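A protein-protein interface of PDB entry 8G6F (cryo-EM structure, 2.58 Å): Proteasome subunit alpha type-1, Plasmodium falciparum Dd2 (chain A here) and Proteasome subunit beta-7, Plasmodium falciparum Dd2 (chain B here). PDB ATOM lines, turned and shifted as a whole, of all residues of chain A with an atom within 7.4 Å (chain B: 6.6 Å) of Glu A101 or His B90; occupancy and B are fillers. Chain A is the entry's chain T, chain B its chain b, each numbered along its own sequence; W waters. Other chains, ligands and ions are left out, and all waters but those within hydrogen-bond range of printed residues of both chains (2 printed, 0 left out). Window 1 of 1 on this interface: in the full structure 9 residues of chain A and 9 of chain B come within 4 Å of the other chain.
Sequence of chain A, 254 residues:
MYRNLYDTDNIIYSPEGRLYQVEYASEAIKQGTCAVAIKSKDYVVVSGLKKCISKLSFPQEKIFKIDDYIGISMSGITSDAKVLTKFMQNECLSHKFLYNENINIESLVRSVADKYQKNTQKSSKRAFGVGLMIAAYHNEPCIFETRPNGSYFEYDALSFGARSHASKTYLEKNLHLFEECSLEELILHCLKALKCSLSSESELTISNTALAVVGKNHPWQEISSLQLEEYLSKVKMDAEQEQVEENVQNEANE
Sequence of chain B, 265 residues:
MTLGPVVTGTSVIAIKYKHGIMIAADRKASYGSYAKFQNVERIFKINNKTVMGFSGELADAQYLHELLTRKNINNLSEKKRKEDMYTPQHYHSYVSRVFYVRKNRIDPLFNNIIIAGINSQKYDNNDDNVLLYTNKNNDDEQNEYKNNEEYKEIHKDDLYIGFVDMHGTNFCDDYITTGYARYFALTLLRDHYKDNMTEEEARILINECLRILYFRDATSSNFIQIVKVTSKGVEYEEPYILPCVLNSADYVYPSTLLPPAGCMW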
ATOM      1  N   ASP A  67       7.062  -8.178 -17.387  1.00  0.00           N
ATOM      2  CA  ASP A  67       7.667  -9.481 -17.612  1.00  0.00           C
ATOM      3  C   ASP A  67       6.557 -10.454 -17.988  1.00  0.00           C
ATOM      4  O   ASP A  67       5.414 -10.054 -18.221  1.00  0.00           O
ATOM      5  CB  ASP A  67       8.443  -9.933 -16.369  1.00  0.00           C
ATOM      6  CG  ASP A  67       9.543 -10.921 -16.692  1.00  0.00           C
ATOM      7  OD1 ASP A  67       9.588 -11.414 -17.837  1.00  0.00           O
ATOM      8  OD2 ASP A  67      10.359 -11.218 -15.794  1.00  0.00           O
ATOM      9  N   CYS A  92      13.981  -7.050 -14.692  1.00  0.00           N
ATOM     10  CA  CYS A  92      13.496  -8.410 -14.898  1.00  0.00           C
ATOM     11  C   CYS A  92      14.323  -9.134 -15.953  1.00  0.00           C
ATOM     12  O   CYS A  92      14.719 -10.293 -15.761  1.00  0.00           O
ATOM     13  CB  CYS A  92      12.024  -8.385 -15.300  1.00  0.00           C
ATOM     14  SG  CYS A  92      10.907  -7.822 -14.007  1.00  0.00           S
ATOM     15  N   LEU A  93      14.606  -8.463 -17.070  1.00  0.00           N
ATOM     16  CA  LEU A  93      15.369  -9.101 -18.135  1.00  0.00           C
ATOM     17  C   LEU A  93      16.786  -9.424 -17.687  1.00  0.00           C
ATOM     18  O   LEU A  93      17.315 -10.490 -18.014  1.00  0.00           O
ATOM     19  CB  LEU A  93      15.389  -8.206 -19.371  1.00  0.00           C
ATOM     20  CG  LEU A  93      14.093  -8.195 -20.178  1.00  0.00           C
ATOM     21  CD1 LEU A  93      14.066  -7.008 -21.114  1.00  0.00           C
ATOM     22  CD2 LEU A  93      13.928  -9.486 -20.945  1.00  0.00           C
ATOM     23  N   SER A  94      17.422  -8.518 -16.945  1.00  0.00           N
ATOM     24  CA  SER A  94      18.783  -8.762 -16.494  1.00  0.00           C
ATOM     25  C   SER A  94      18.839  -9.876 -15.462  1.00  0.00           C
ATOM     26  O   SER A  94      19.798 -10.651 -15.446  1.00  0.00           O
ATOM     27  CB  SER A  94      19.387  -7.479 -15.927  1.00  0.00           C
ATOM     28  OG  SER A  94      19.111  -7.351 -14.547  1.00  0.00           O
ATOM     29  N   HIS A  95      17.832  -9.984 -14.596  1.00  0.00           N
ATOM     30  CA  HIS A  95      17.791 -11.125 -13.692  1.00  0.00           C
ATOM     31  C   HIS A  95      17.654 -12.428 -14.466  1.00  0.00           C
ATOM     32  O   HIS A  95      18.329 -13.416 -14.157  1.00  0.00           O
ATOM     33  CB  HIS A  95      16.646 -10.978 -12.695  1.00  0.00           C
ATOM     34  CG  HIS A  95      16.722 -11.940 -11.553  1.00  0.00           C
ATOM     35  ND1 HIS A  95      17.318 -11.624 -10.354  1.00  0.00           N
ATOM     36  CD2 HIS A  95      16.291 -13.217 -11.435  1.00  0.00           C
ATOM     37  CE1 HIS A  95      17.241 -12.661  -9.540  1.00  0.00           C
ATOM     38  NE2 HIS A  95      16.623 -13.640 -10.173  1.00  0.00           N
ATOM     39  N   LYS A  96      16.785 -12.452 -15.477  1.00  0.00           N
ATOM     40  CA  LYS A  96      16.649 -13.660 -16.285  1.00  0.00           C
ATOM     41  C   LYS A  96      17.957 -13.997 -16.988  1.00  0.00           C
ATOM     42  O   LYS A  96      18.325 -15.170 -17.107  1.00  0.00           O
ATOM     43  CB  LYS A  96      15.526 -13.487 -17.304  1.00  0.00           C
ATOM     44  CG  LYS A  96      14.169 -13.899 -16.781  1.00  0.00           C
ATOM     45  CD  LYS A  96      13.071 -13.622 -17.784  1.00  0.00           C
ATOM     46  CE  LYS A  96      11.709 -13.972 -17.213  1.00  0.00           C
ATOM     47  NZ  LYS A  96      10.597 -13.606 -18.132  1.00  0.00           N
ATOM     48  N   PHE A  97      18.668 -12.978 -17.464  1.00  0.00           N
ATOM     49  CA  PHE A  97      19.943 -13.196 -18.136  1.00  0.00           C
ATOM     50  C   PHE A  97      20.987 -13.759 -17.179  1.00  0.00           C
ATOM     51  O   PHE A  97      21.705 -14.707 -17.515  1.00  0.00           O
ATOM     52  CB  PHE A  97      20.426 -11.881 -18.745  1.00  0.00           C
ATOM     53  CG  PHE A  97      21.849 -11.911 -19.216  1.00  0.00           C
ATOM     54  CD1 PHE A  97      22.184 -12.518 -20.411  1.00  0.00           C
ATOM     55  CD2 PHE A  97      22.849 -11.311 -18.475  1.00  0.00           C
ATOM     56  CE1 PHE A  97      23.487 -12.538 -20.848  1.00  0.00           C
ATOM     57  CE2 PHE A  97      24.155 -11.329 -18.910  1.00  0.00           C
ATOM     58  CZ  PHE A  97      24.474 -11.944 -20.099  1.00  0.00           C
ATOM     59  N   LEU A  98      21.089 -13.187 -15.979  1.00  0.00           N
ATOM     60  CA  LEU A  98      22.159 -13.565 -15.065  1.00  0.00           C
ATOM     61  C   LEU A  98      21.896 -14.904 -14.388  1.00  0.00           C
ATOM     62  O   LEU A  98      22.825 -15.696 -14.205  1.00  0.00           O
ATOM     63  CB  LEU A  98      22.354 -12.480 -14.008  1.00  0.00           C
ATOM     64  CG  LEU A  98      22.934 -11.150 -14.479  1.00  0.00           C
ATOM     65  CD1 LEU A  98      22.983 -10.175 -13.324  1.00  0.00           C
ATOM     66  CD2 LEU A  98      24.314 -11.328 -15.078  1.00  0.00           C
ATOM     67  N   TYR A  99      20.650 -15.176 -14.004  1.00  0.00           N
ATOM     68  CA  TYR A  99      20.339 -16.331 -13.176  1.00  0.00           C
ATOM     69  C   TYR A  99      19.401 -17.325 -13.837  1.00  0.00           C
ATOM     70  O   TYR A  99      19.113 -18.365 -13.238  1.00  0.00           O
ATOM     71  CB  TYR A  99      19.733 -15.875 -11.846  1.00  0.00           C
ATOM     72  CG  TYR A  99      20.617 -14.916 -11.094  1.00  0.00           C
ATOM     73  CD1 TYR A  99      21.763 -15.360 -10.452  1.00  0.00           C
ATOM     74  CD2 TYR A  99      20.318 -13.566 -11.039  1.00  0.00           C
ATOM     75  CE1 TYR A  99      22.575 -14.489  -9.771  1.00  0.00           C
ATOM     76  CE2 TYR A  99      21.125 -12.689 -10.361  1.00  0.00           C
ATOM     77  CZ  TYR A  99      22.250 -13.153  -9.727  1.00  0.00           C
ATOM     78  OH  TYR A  99      23.057 -12.275  -9.047  1.00  0.00           O
ATOM     79  N   ASN A 100      18.921 -17.049 -15.043  1.00  0.00           N
ATOM     80  CA  ASN A 100      18.065 -17.984 -15.765  1.00  0.00           C
ATOM     81  C   ASN A 100      16.845 -18.366 -14.932  1.00  0.00           C
ATOM     82  O   ASN A 100      16.479 -19.537 -14.833  1.00  0.00           O
ATOM     83  CB  ASN A 100      18.851 -19.231 -16.180  1.00  0.00           C
ATOM     84  CG  ASN A 100      20.295 -18.920 -16.533  1.00  0.00           C
ATOM     85  OD1 ASN A 100      21.220 -19.492 -15.966  1.00  0.00           O
ATOM     86  ND2 ASN A 100      20.492 -18.006 -17.474  1.00  0.00           N
ATOM     87  N   GLU A 101      16.216 -17.368 -14.319  1.00  0.00           N
ATOM     88  CA  GLU A 101      15.010 -17.591 -13.536  1.00  0.00           C
ATOM     89  C   GLU A 101      14.282 -16.266 -13.381  1.00  0.00           C
ATOM     90  O   GLU A 101      14.846 -15.197 -13.615  1.00  0.00           O
ATOM     91  CB  GLU A 101      15.333 -18.193 -12.168  1.00  0.00           C
ATOM     92  CG  GLU A 101      16.448 -17.476 -11.440  1.00  0.00           C
ATOM     93  CD  GLU A 101      16.414 -17.705  -9.952  1.00  0.00           C
ATOM     94  OE1 GLU A 101      16.131 -18.845  -9.536  1.00  0.00           O
ATOM     95  OE2 GLU A 101      16.669 -16.747  -9.195  1.00  0.00           O
ATOM     96  N   ASN A 102      13.017 -16.354 -12.979  1.00  0.00           N
ATOM     97  CA  ASN A 102      12.210 -15.163 -12.761  1.00  0.00           C
ATOM     98  C   ASN A 102      12.686 -14.408 -11.529  1.00  0.00           C
ATOM     99  O   ASN A 102      13.079 -15.007 -10.525  1.00  0.00           O
ATOM    100  CB  ASN A 102      10.742 -15.540 -12.587  1.00  0.00           C
ATOM    101  CG  ASN A 102      10.117 -16.049 -13.859  1.00  0.00           C
ATOM    102  OD1 ASN A 102      10.585 -15.758 -14.957  1.00  0.00           O
ATOM    103  ND2 ASN A 102       9.045 -16.818 -13.719  1.00  0.00           N
ATOM    104  N   ILE A 103      12.638 -13.079 -11.606  1.00  0.00           N
ATOM    105  CA  ILE A 103      13.017 -12.254 -10.468  1.00  0.00           C
ATOM    106  C   ILE A 103      11.955 -12.360  -9.382  1.00  0.00           C
ATOM    107  O   ILE A 103      10.769 -12.584  -9.654  1.00  0.00           O
ATOM    108  CB  ILE A 103      13.216 -10.792 -10.904  1.00  0.00           C
ATOM    109  CG1 ILE A 103      13.877  -9.989  -9.783  1.00  0.00           C
ATOM    110  CG2 ILE A 103      11.886 -10.167 -11.286  1.00  0.00           C
ATOM    111  CD1 ILE A 103      14.180  -8.561 -10.151  1.00  0.00           C
ATOM    112  N   ASN A 104      12.387 -12.201  -8.138  1.00  0.00           N
ATOM    113  CA  ASN A 104      11.456 -12.134  -7.023  1.00  0.00           C
ATOM    114  C   ASN A 104      10.734 -10.793  -7.041  1.00  0.00           C
ATOM    115  O   ASN A 104      11.365  -9.731  -7.068  1.00  0.00           O
ATOM    116  CB  ASN A 104      12.207 -12.329  -5.710  1.00  0.00           C
ATOM    117  CG  ASN A 104      11.286 -12.454  -4.524  1.00  0.00           C
ATOM    118  OD1 ASN A 104      10.283 -13.159  -4.573  1.00  0.00           O
ATOM    119  ND2 ASN A 104      11.628 -11.776  -3.442  1.00  0.00           N
ATOM    120  N   HIS A 138       3.957 -14.730  -8.585  1.00  0.00           N
ATOM    121  CA  HIS A 138       5.204 -15.387  -8.190  1.00  0.00           C
ATOM    122  C   HIS A 138       4.855 -16.334  -7.042  1.00  0.00           C
ATOM    123  O   HIS A 138       4.889 -15.943  -5.873  1.00  0.00           O
ATOM    124  CB  HIS A 138       6.262 -14.369  -7.787  1.00  0.00           C
ATOM    125  CG  HIS A 138       7.656 -14.912  -7.796  1.00  0.00           C
ATOM    126  ND1 HIS A 138       8.457 -14.920  -6.674  1.00  0.00           N
ATOM    127  CD2 HIS A 138       8.391 -15.466  -8.787  1.00  0.00           C
ATOM    128  CE1 HIS A 138       9.625 -15.457  -6.976  1.00  0.00           C
ATOM    129  NE2 HIS A 138       9.611 -15.795  -8.252  1.00  0.00           N
ATOM    130  N   LYS B  71      26.536 -13.636  -0.154  1.00  0.00           N
ATOM    131  CA  LYS B  71      25.325 -13.723  -0.959  1.00  0.00           C
ATOM    132  C   LYS B  71      24.210 -14.415  -0.188  1.00  0.00           C
ATOM    133  O   LYS B  71      23.056 -13.966  -0.203  1.00  0.00           O
ATOM    134  CB  LYS B  71      25.625 -14.463  -2.258  1.00  0.00           C
ATOM    135  CG  LYS B  71      24.452 -14.557  -3.192  1.00  0.00           C
ATOM    136  CD  LYS B  71      24.883 -15.002  -4.562  1.00  0.00           C
ATOM    137  CE  LYS B  71      23.724 -14.978  -5.522  1.00  0.00           C
ATOM    138  NZ  LYS B  71      23.362 -13.590  -5.891  1.00  0.00           N
ATOM    139  N   TYR B  86      17.624 -18.845  -2.178  1.00  0.00           N
ATOM    140  CA  TYR B  86      18.232 -19.141  -3.465  1.00  0.00           C
ATOM    141  C   TYR B  86      18.466 -20.635  -3.620  1.00  0.00           C
ATOM    142  O   TYR B  86      18.656 -21.366  -2.644  1.00  0.00           O
ATOM    143  CB  TYR B  86      19.557 -18.401  -3.614  1.00  0.00           C
ATOM    144  CG  TYR B  86      19.432 -16.903  -3.736  1.00  0.00           C
ATOM    145  CD1 TYR B  86      18.288 -16.319  -4.254  1.00  0.00           C
ATOM    146  CD2 TYR B  86      20.467 -16.072  -3.341  1.00  0.00           C
ATOM    147  CE1 TYR B  86      18.176 -14.956  -4.369  1.00  0.00           C
ATOM    148  CE2 TYR B  86      20.364 -14.707  -3.454  1.00  0.00           C
ATOM    149  CZ  TYR B  86      19.215 -14.154  -3.968  1.00  0.00           C
ATOM    150  OH  TYR B  86      19.102 -12.792  -4.082  1.00  0.00           O
ATOM    151  N   THR B  87      18.465 -21.081  -4.859  1.00  0.00           N
ATOM    152  CA  THR B  87      18.586 -22.489  -5.177  1.00  0.00           C
ATOM    153  C   THR B  87      19.991 -22.826  -5.654  1.00  0.00           C
ATOM    154  O   THR B  87      20.777 -21.940  -6.011  1.00  0.00           O
ATOM    155  CB  THR B  87      17.576 -22.880  -6.258  1.00  0.00           C
ATOM    156  OG1 THR B  87      17.714 -22.012  -7.386  1.00  0.00           O
ATOM    157  CG2 THR B  87      16.169 -22.776  -5.723  1.00  0.00           C
ATOM    158  N   PRO B  88      20.340 -24.113  -5.662  1.00  0.00           N
ATOM    159  CA  PRO B  88      21.623 -24.503  -6.259  1.00  0.00           C
ATOM    160  C   PRO B  88      21.763 -24.055  -7.699  1.00  0.00           C
ATOM    161  O   PRO B  88      22.866 -23.699  -8.117  1.00  0.00           O
ATOM    162  CB  PRO B  88      21.614 -26.033  -6.132  1.00  0.00           C
ATOM    163  CG  PRO B  88      20.694 -26.314  -5.022  1.00  0.00           C
ATOM    164  CD  PRO B  88      19.643 -25.259  -5.059  1.00  0.00           C
ATOM    165  N   GLN B  89      20.678 -24.059  -8.473  1.00  0.00           N
ATOM    166  CA  GLN B  89      20.754 -23.549  -9.837  1.00  0.00           C
ATOM    167  C   GLN B  89      21.123 -22.072  -9.848  1.00  0.00           C
ATOM    168  O   GLN B  89      21.933 -21.631 -10.670  1.00  0.00           O
ATOM    169  CB  GLN B  89      19.423 -23.773 -10.555  1.00  0.00           C
ATOM    170  CG  GLN B  89      19.459 -23.452 -12.040  1.00  0.00           C
ATOM    171  CD  GLN B  89      19.195 -21.986 -12.340  1.00  0.00           C
ATOM    172  OE1 GLN B  89      18.346 -21.352 -11.717  1.00  0.00           O
ATOM    173  NE2 GLN B  89      19.930 -21.439 -13.296  1.00  0.00           N
ATOM    174  N   HIS B  90      20.530 -21.289  -8.948  1.00  0.00           N
ATOM    175  CA  HIS B  90      20.846 -19.869  -8.868  1.00  0.00           C
ATOM    176  C   HIS B  90      22.316 -19.656  -8.534  1.00  0.00           C
ATOM    177  O   HIS B  90      22.996 -18.827  -9.151  1.00  0.00           O
ATOM    178  CB  HIS B  90      19.941 -19.210  -7.825  1.00  0.00           C
ATOM    179  CG  HIS B  90      20.248 -17.768  -7.564  1.00  0.00           C
ATOM    180  ND1 HIS B  90      19.442 -16.744  -8.009  1.00  0.00           N
ATOM    181  CD2 HIS B  90      21.254 -17.181  -6.875  1.00  0.00           C
ATOM    182  CE1 HIS B  90      19.948 -15.588  -7.621  1.00  0.00           C
ATOM    183  NE2 HIS B  90      21.049 -15.826  -6.934  1.00  0.00           N
ATOM    184  N   TYR B  91      22.830 -20.405  -7.560  1.00  0.00           N
ATOM    185  CA  TYR B  91      24.236 -20.253  -7.197  1.00  0.00           C
ATOM    186  C   TYR B  91      25.155 -20.723  -8.321  1.00  0.00           C
ATOM    187  O   TYR B  91      26.223 -20.141  -8.540  1.00  0.00           O
ATOM    188  CB  TYR B  91      24.525 -21.010  -5.905  1.00  0.00           C
ATOM    189  CG  TYR B  91      24.080 -20.270  -4.669  1.00  0.00           C
ATOM    190  CD1 TYR B  91      24.798 -19.185  -4.191  1.00  0.00           C
ATOM    191  CD2 TYR B  91      22.946 -20.656  -3.976  1.00  0.00           C
ATOM    192  CE1 TYR B  91      24.397 -18.508  -3.064  1.00  0.00           C
ATOM    193  CE2 TYR B  91      22.538 -19.986  -2.850  1.00  0.00           C
ATOM    194  CZ  TYR B  91      23.267 -18.913  -2.396  1.00  0.00           C
ATOM    195  OH  TYR B  91      22.860 -18.247  -1.271  1.00  0.00           O
ATOM    196  N   HIS B  92      24.766 -21.778  -9.035  1.00  0.00           N
ATOM    197  CA  HIS B  92      25.554 -22.237 -10.172  1.00  0.00           C
ATOM    198  C   HIS B  92      25.620 -21.169 -11.253  1.00  0.00           C
ATOM    199  O   HIS B  92      26.684 -20.921 -11.827  1.00  0.00           O
ATOM    200  CB  HIS B  92      24.958 -23.533 -10.719  1.00  0.00           C
ATOM    201  CG  HIS B  92      25.747 -24.143 -11.835  1.00  0.00           C
ATOM    202  ND1 HIS B  92      25.181 -24.493 -13.040  1.00  0.00           N
ATOM    203  CD2 HIS B  92      27.057 -24.467 -11.929  1.00  0.00           C
ATOM    204  CE1 HIS B  92      26.107 -25.006 -13.828  1.00  0.00           C
ATOM    205  NE2 HIS B  92      27.255 -24.998 -13.177  1.00  0.00           N
ATOM    206  N   SER B  93      24.492 -20.515 -11.532  1.00  0.00           N
ATOM    207  CA  SER B  93      24.491 -19.421 -12.496  1.00  0.00           C
ATOM    208  C   SER B  93      25.379 -18.277 -12.029  1.00  0.00           C
ATOM    209  O   SER B  93      26.120 -17.688 -12.825  1.00  0.00           O
ATOM    210  CB  SER B  93      23.067 -18.929 -12.721  1.00  0.00           C
ATOM    211  OG  SER B  93      22.324 -19.870 -13.464  1.00  0.00           O
ATOM    212  N   TYR B  94      25.320 -17.947 -10.740  1.00  0.00           N
ATOM    213  CA  TYR B  94      26.156 -16.877 -10.209  1.00  0.00           C
ATOM    214  C   TYR B  94      27.637 -17.191 -10.392  1.00  0.00           C
ATOM    215  O   TYR B  94      28.413 -16.349 -10.861  1.00  0.00           O
ATOM    216  CB  TYR B  94      25.827 -16.661  -8.733  1.00  0.00           C
ATOM    217  CG  TYR B  94      26.651 -15.588  -8.076  1.00  0.00           C
ATOM    218  CD1 TYR B  94      26.488 -14.259  -8.422  1.00  0.00           C
ATOM    219  CD2 TYR B  94      27.594 -15.902  -7.115  1.00  0.00           C
ATOM    220  CE1 TYR B  94      27.236 -13.277  -7.831  1.00  0.00           C
ATOM    221  CE2 TYR B  94      28.348 -14.925  -6.518  1.00  0.00           C
ATOM    222  CZ  TYR B  94      28.163 -13.612  -6.879  1.00  0.00           C
ATOM    223  OH  TYR B  94      28.915 -12.628  -6.288  1.00  0.00           O
ATOM    224  N   VAL B  95      28.045 -18.409 -10.040  1.00  0.00           N
ATOM    225  CA  VAL B  95      29.451 -18.783 -10.144  1.00  0.00           C
ATOM    226  C   VAL B  95      29.887 -18.827 -11.603  1.00  0.00           C
ATOM    227  O   VAL B  95      31.009 -18.432 -11.943  1.00  0.00           O
ATOM    228  CB  VAL B  95      29.692 -20.125  -9.432  1.00  0.00           C
ATOM    229  CG1 VAL B  95      31.049 -20.693  -9.792  1.00  0.00           C
ATOM    230  CG2 VAL B  95      29.576 -19.944  -7.936  1.00  0.00           C
ATOM    231  N   ILE B 115      28.760 -27.099  -7.694  1.00  0.00           N
ATOM    232  CA  ILE B 115      27.669 -26.546  -6.897  1.00  0.00           C
ATOM    233  C   ILE B 115      26.563 -27.588  -6.872  1.00  0.00           C
ATOM    234  O   ILE B 115      25.970 -27.891  -7.911  1.00  0.00           O
ATOM    235  CB  ILE B 115      27.155 -25.218  -7.471  1.00  0.00           C
ATOM    236  CG1 ILE B 115      28.272 -24.173  -7.532  1.00  0.00           C
ATOM    237  CG2 ILE B 115      25.987 -24.706  -6.647  1.00  0.00           C
ATOM    238  CD1 ILE B 115      28.630 -23.567  -6.204  1.00  0.00           C
ATOM    239  N   ASN B 119      17.037 -28.652  -5.329  1.00  0.00           N
ATOM    240  CA  ASN B 119      16.427 -27.577  -6.098  1.00  0.00           C
ATOM    241  C   ASN B 119      14.946 -27.406  -5.791  1.00  0.00           C
ATOM    242  O   ASN B 119      14.180 -26.987  -6.665  1.00  0.00           O
ATOM    243  CB  ASN B 119      16.634 -27.842  -7.590  1.00  0.00           C
ATOM    244  CG  ASN B 119      17.161 -26.636  -8.332  1.00  0.00           C
ATOM    245  OD1 ASN B 119      17.957 -25.868  -7.803  1.00  0.00           O
ATOM    246  ND2 ASN B 119      16.727 -26.471  -9.571  1.00  0.00           N
ATOM    247  N   TYR B 160      20.186 -31.226  -7.875  1.00  0.00           N
ATOM    248  CA  TYR B 160      20.994 -30.421  -8.777  1.00  0.00           C
ATOM    249  C   TYR B 160      22.468 -30.601  -8.457  1.00  0.00           C
ATOM    250  O   TYR B 160      22.886 -30.411  -7.313  1.00  0.00           O
ATOM    251  CB  TYR B 160      20.608 -28.944  -8.672  1.00  0.00           C
ATOM    252  CG  TYR B 160      21.279 -28.072  -9.696  1.00  0.00           C
ATOM    253  CD1 TYR B 160      20.762 -27.949 -10.971  1.00  0.00           C
ATOM    254  CD2 TYR B 160      22.433 -27.374  -9.389  1.00  0.00           C
ATOM    255  CE1 TYR B 160      21.372 -27.158 -11.906  1.00  0.00           C
ATOM    256  CE2 TYR B 160      23.049 -26.582 -10.320  1.00  0.00           C
ATOM    257  CZ  TYR B 160      22.514 -26.477 -11.576  1.00  0.00           C
ATOM    258  OH  TYR B 160      23.123 -25.684 -12.513  1.00  0.00           O
HETATM  259  O   HOH W   1      25.149 -17.060 -15.793  1.00  0.00           O
HETATM  260  O   HOH W   2      16.746 -18.902  -6.933  1.00  0.00           O
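Leu A98 touches Ser B93. CE1 of His B90 touches CD1 of Tyr A99, 3.4 Å away. Tyr A99 touches Ser B93. Asn A100 touches Gln B89. Gln B89 touches Glu A101.
A ring nitrogen (NE2) of His B90 sits close to the side-chain amino group (NZ) of Lys B71 (3.4 Å). The backbone NH of His B90 is in hydrogen-bond range of the side-chain hydroxyl of Thr B87 (3.3 Å). The side-chain hydroxyl (OG) of Ser B93 sits at hydrogen-bond distance from the side-chain amide nitrogen (NE2) of Gln B89. The side-chain amide oxygen (OD1) of Asn B119 lies within hydrogen-bond range of the backbone NH (N) of Gln B89 (3.3 Å). OE2 of Glu A101 lies within hydrogen-bond range of NE2 of His A95 (3.3 Å).
The side-chain amino group (NZ) of Lys B71 is in hydrogen-bond range of the side-chain hydroxyl (OH) of Tyr A99 (3.4 Å). The side-chain amide nitrogen (NE2) of Gln B89 is in hydrogen-bond range of the backbone carbonyl oxygen (O) of Tyr A99 (3.2 Å). A ring nitrogen (ND1) of His B90 is in hydrogen-bond range of the side-chain carboxylate (OE2) of Glu A101 (3.0 Å). The side-chain amide oxygen of Asn A100 lies within hydrogen-bond range of the side-chain hydroxyl of Ser B93 (2.8 Å).
Water W2 lies within hydrogen-bond range of the side-chain carboxylate (OE1) of Glu A101 (2.7 Å) and the side-chain hydroxyl (OG1) of Thr B87 (3.3 Å). Water W1 bridges the backbone carbonyl oxygen (O) of Leu A98 (3.1 Å) and the backbone carbonyl oxygen (O) of Ser B93 (3.2 Å).
Of the 15 printed residues of chain A, 4 touch a printed residue of chain B. Hydrophobic or aromatic side chains of chain A that line the printed part of chain B: Tyr A99. Of the 14 printed residues of chain B, 4 touch a printed residue of chain A. Printed residues of chain B that touch a printed residue of chain A: Lys B71, Gln B89, His B90 and Ser B93. Hydrophobic or aromatic side chains of chain B that line the printed part of chain A: His B90. Among the printed residues, no Asp or Glu carboxylate lies within 4 Å of a Lys or Arg side-chain nitrogen of the other chain.
Of the printed residues of chain B, Asn A100 touches Gln B89 (3.5 Å) and Ser B93 (2.8 Å). Printed residues of chain A within 4 Å of Ser B93: Leu A98 (3.6 Å), Tyr A99 (3.6 Å) and Asn A100 (2.8 Å). Printed residues of chain A within 4 Å of Gln B89: Tyr A99, Asn A100 and Glu A101. Of the printed residues of chain A, Lys B71 touches Tyr A99 (3.4 Å). Thr B87 touches none of the printed residues of chain A. The nearest printed residue of chain B that does not touch Glu A101 is Thr B87 (4.1 Å).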
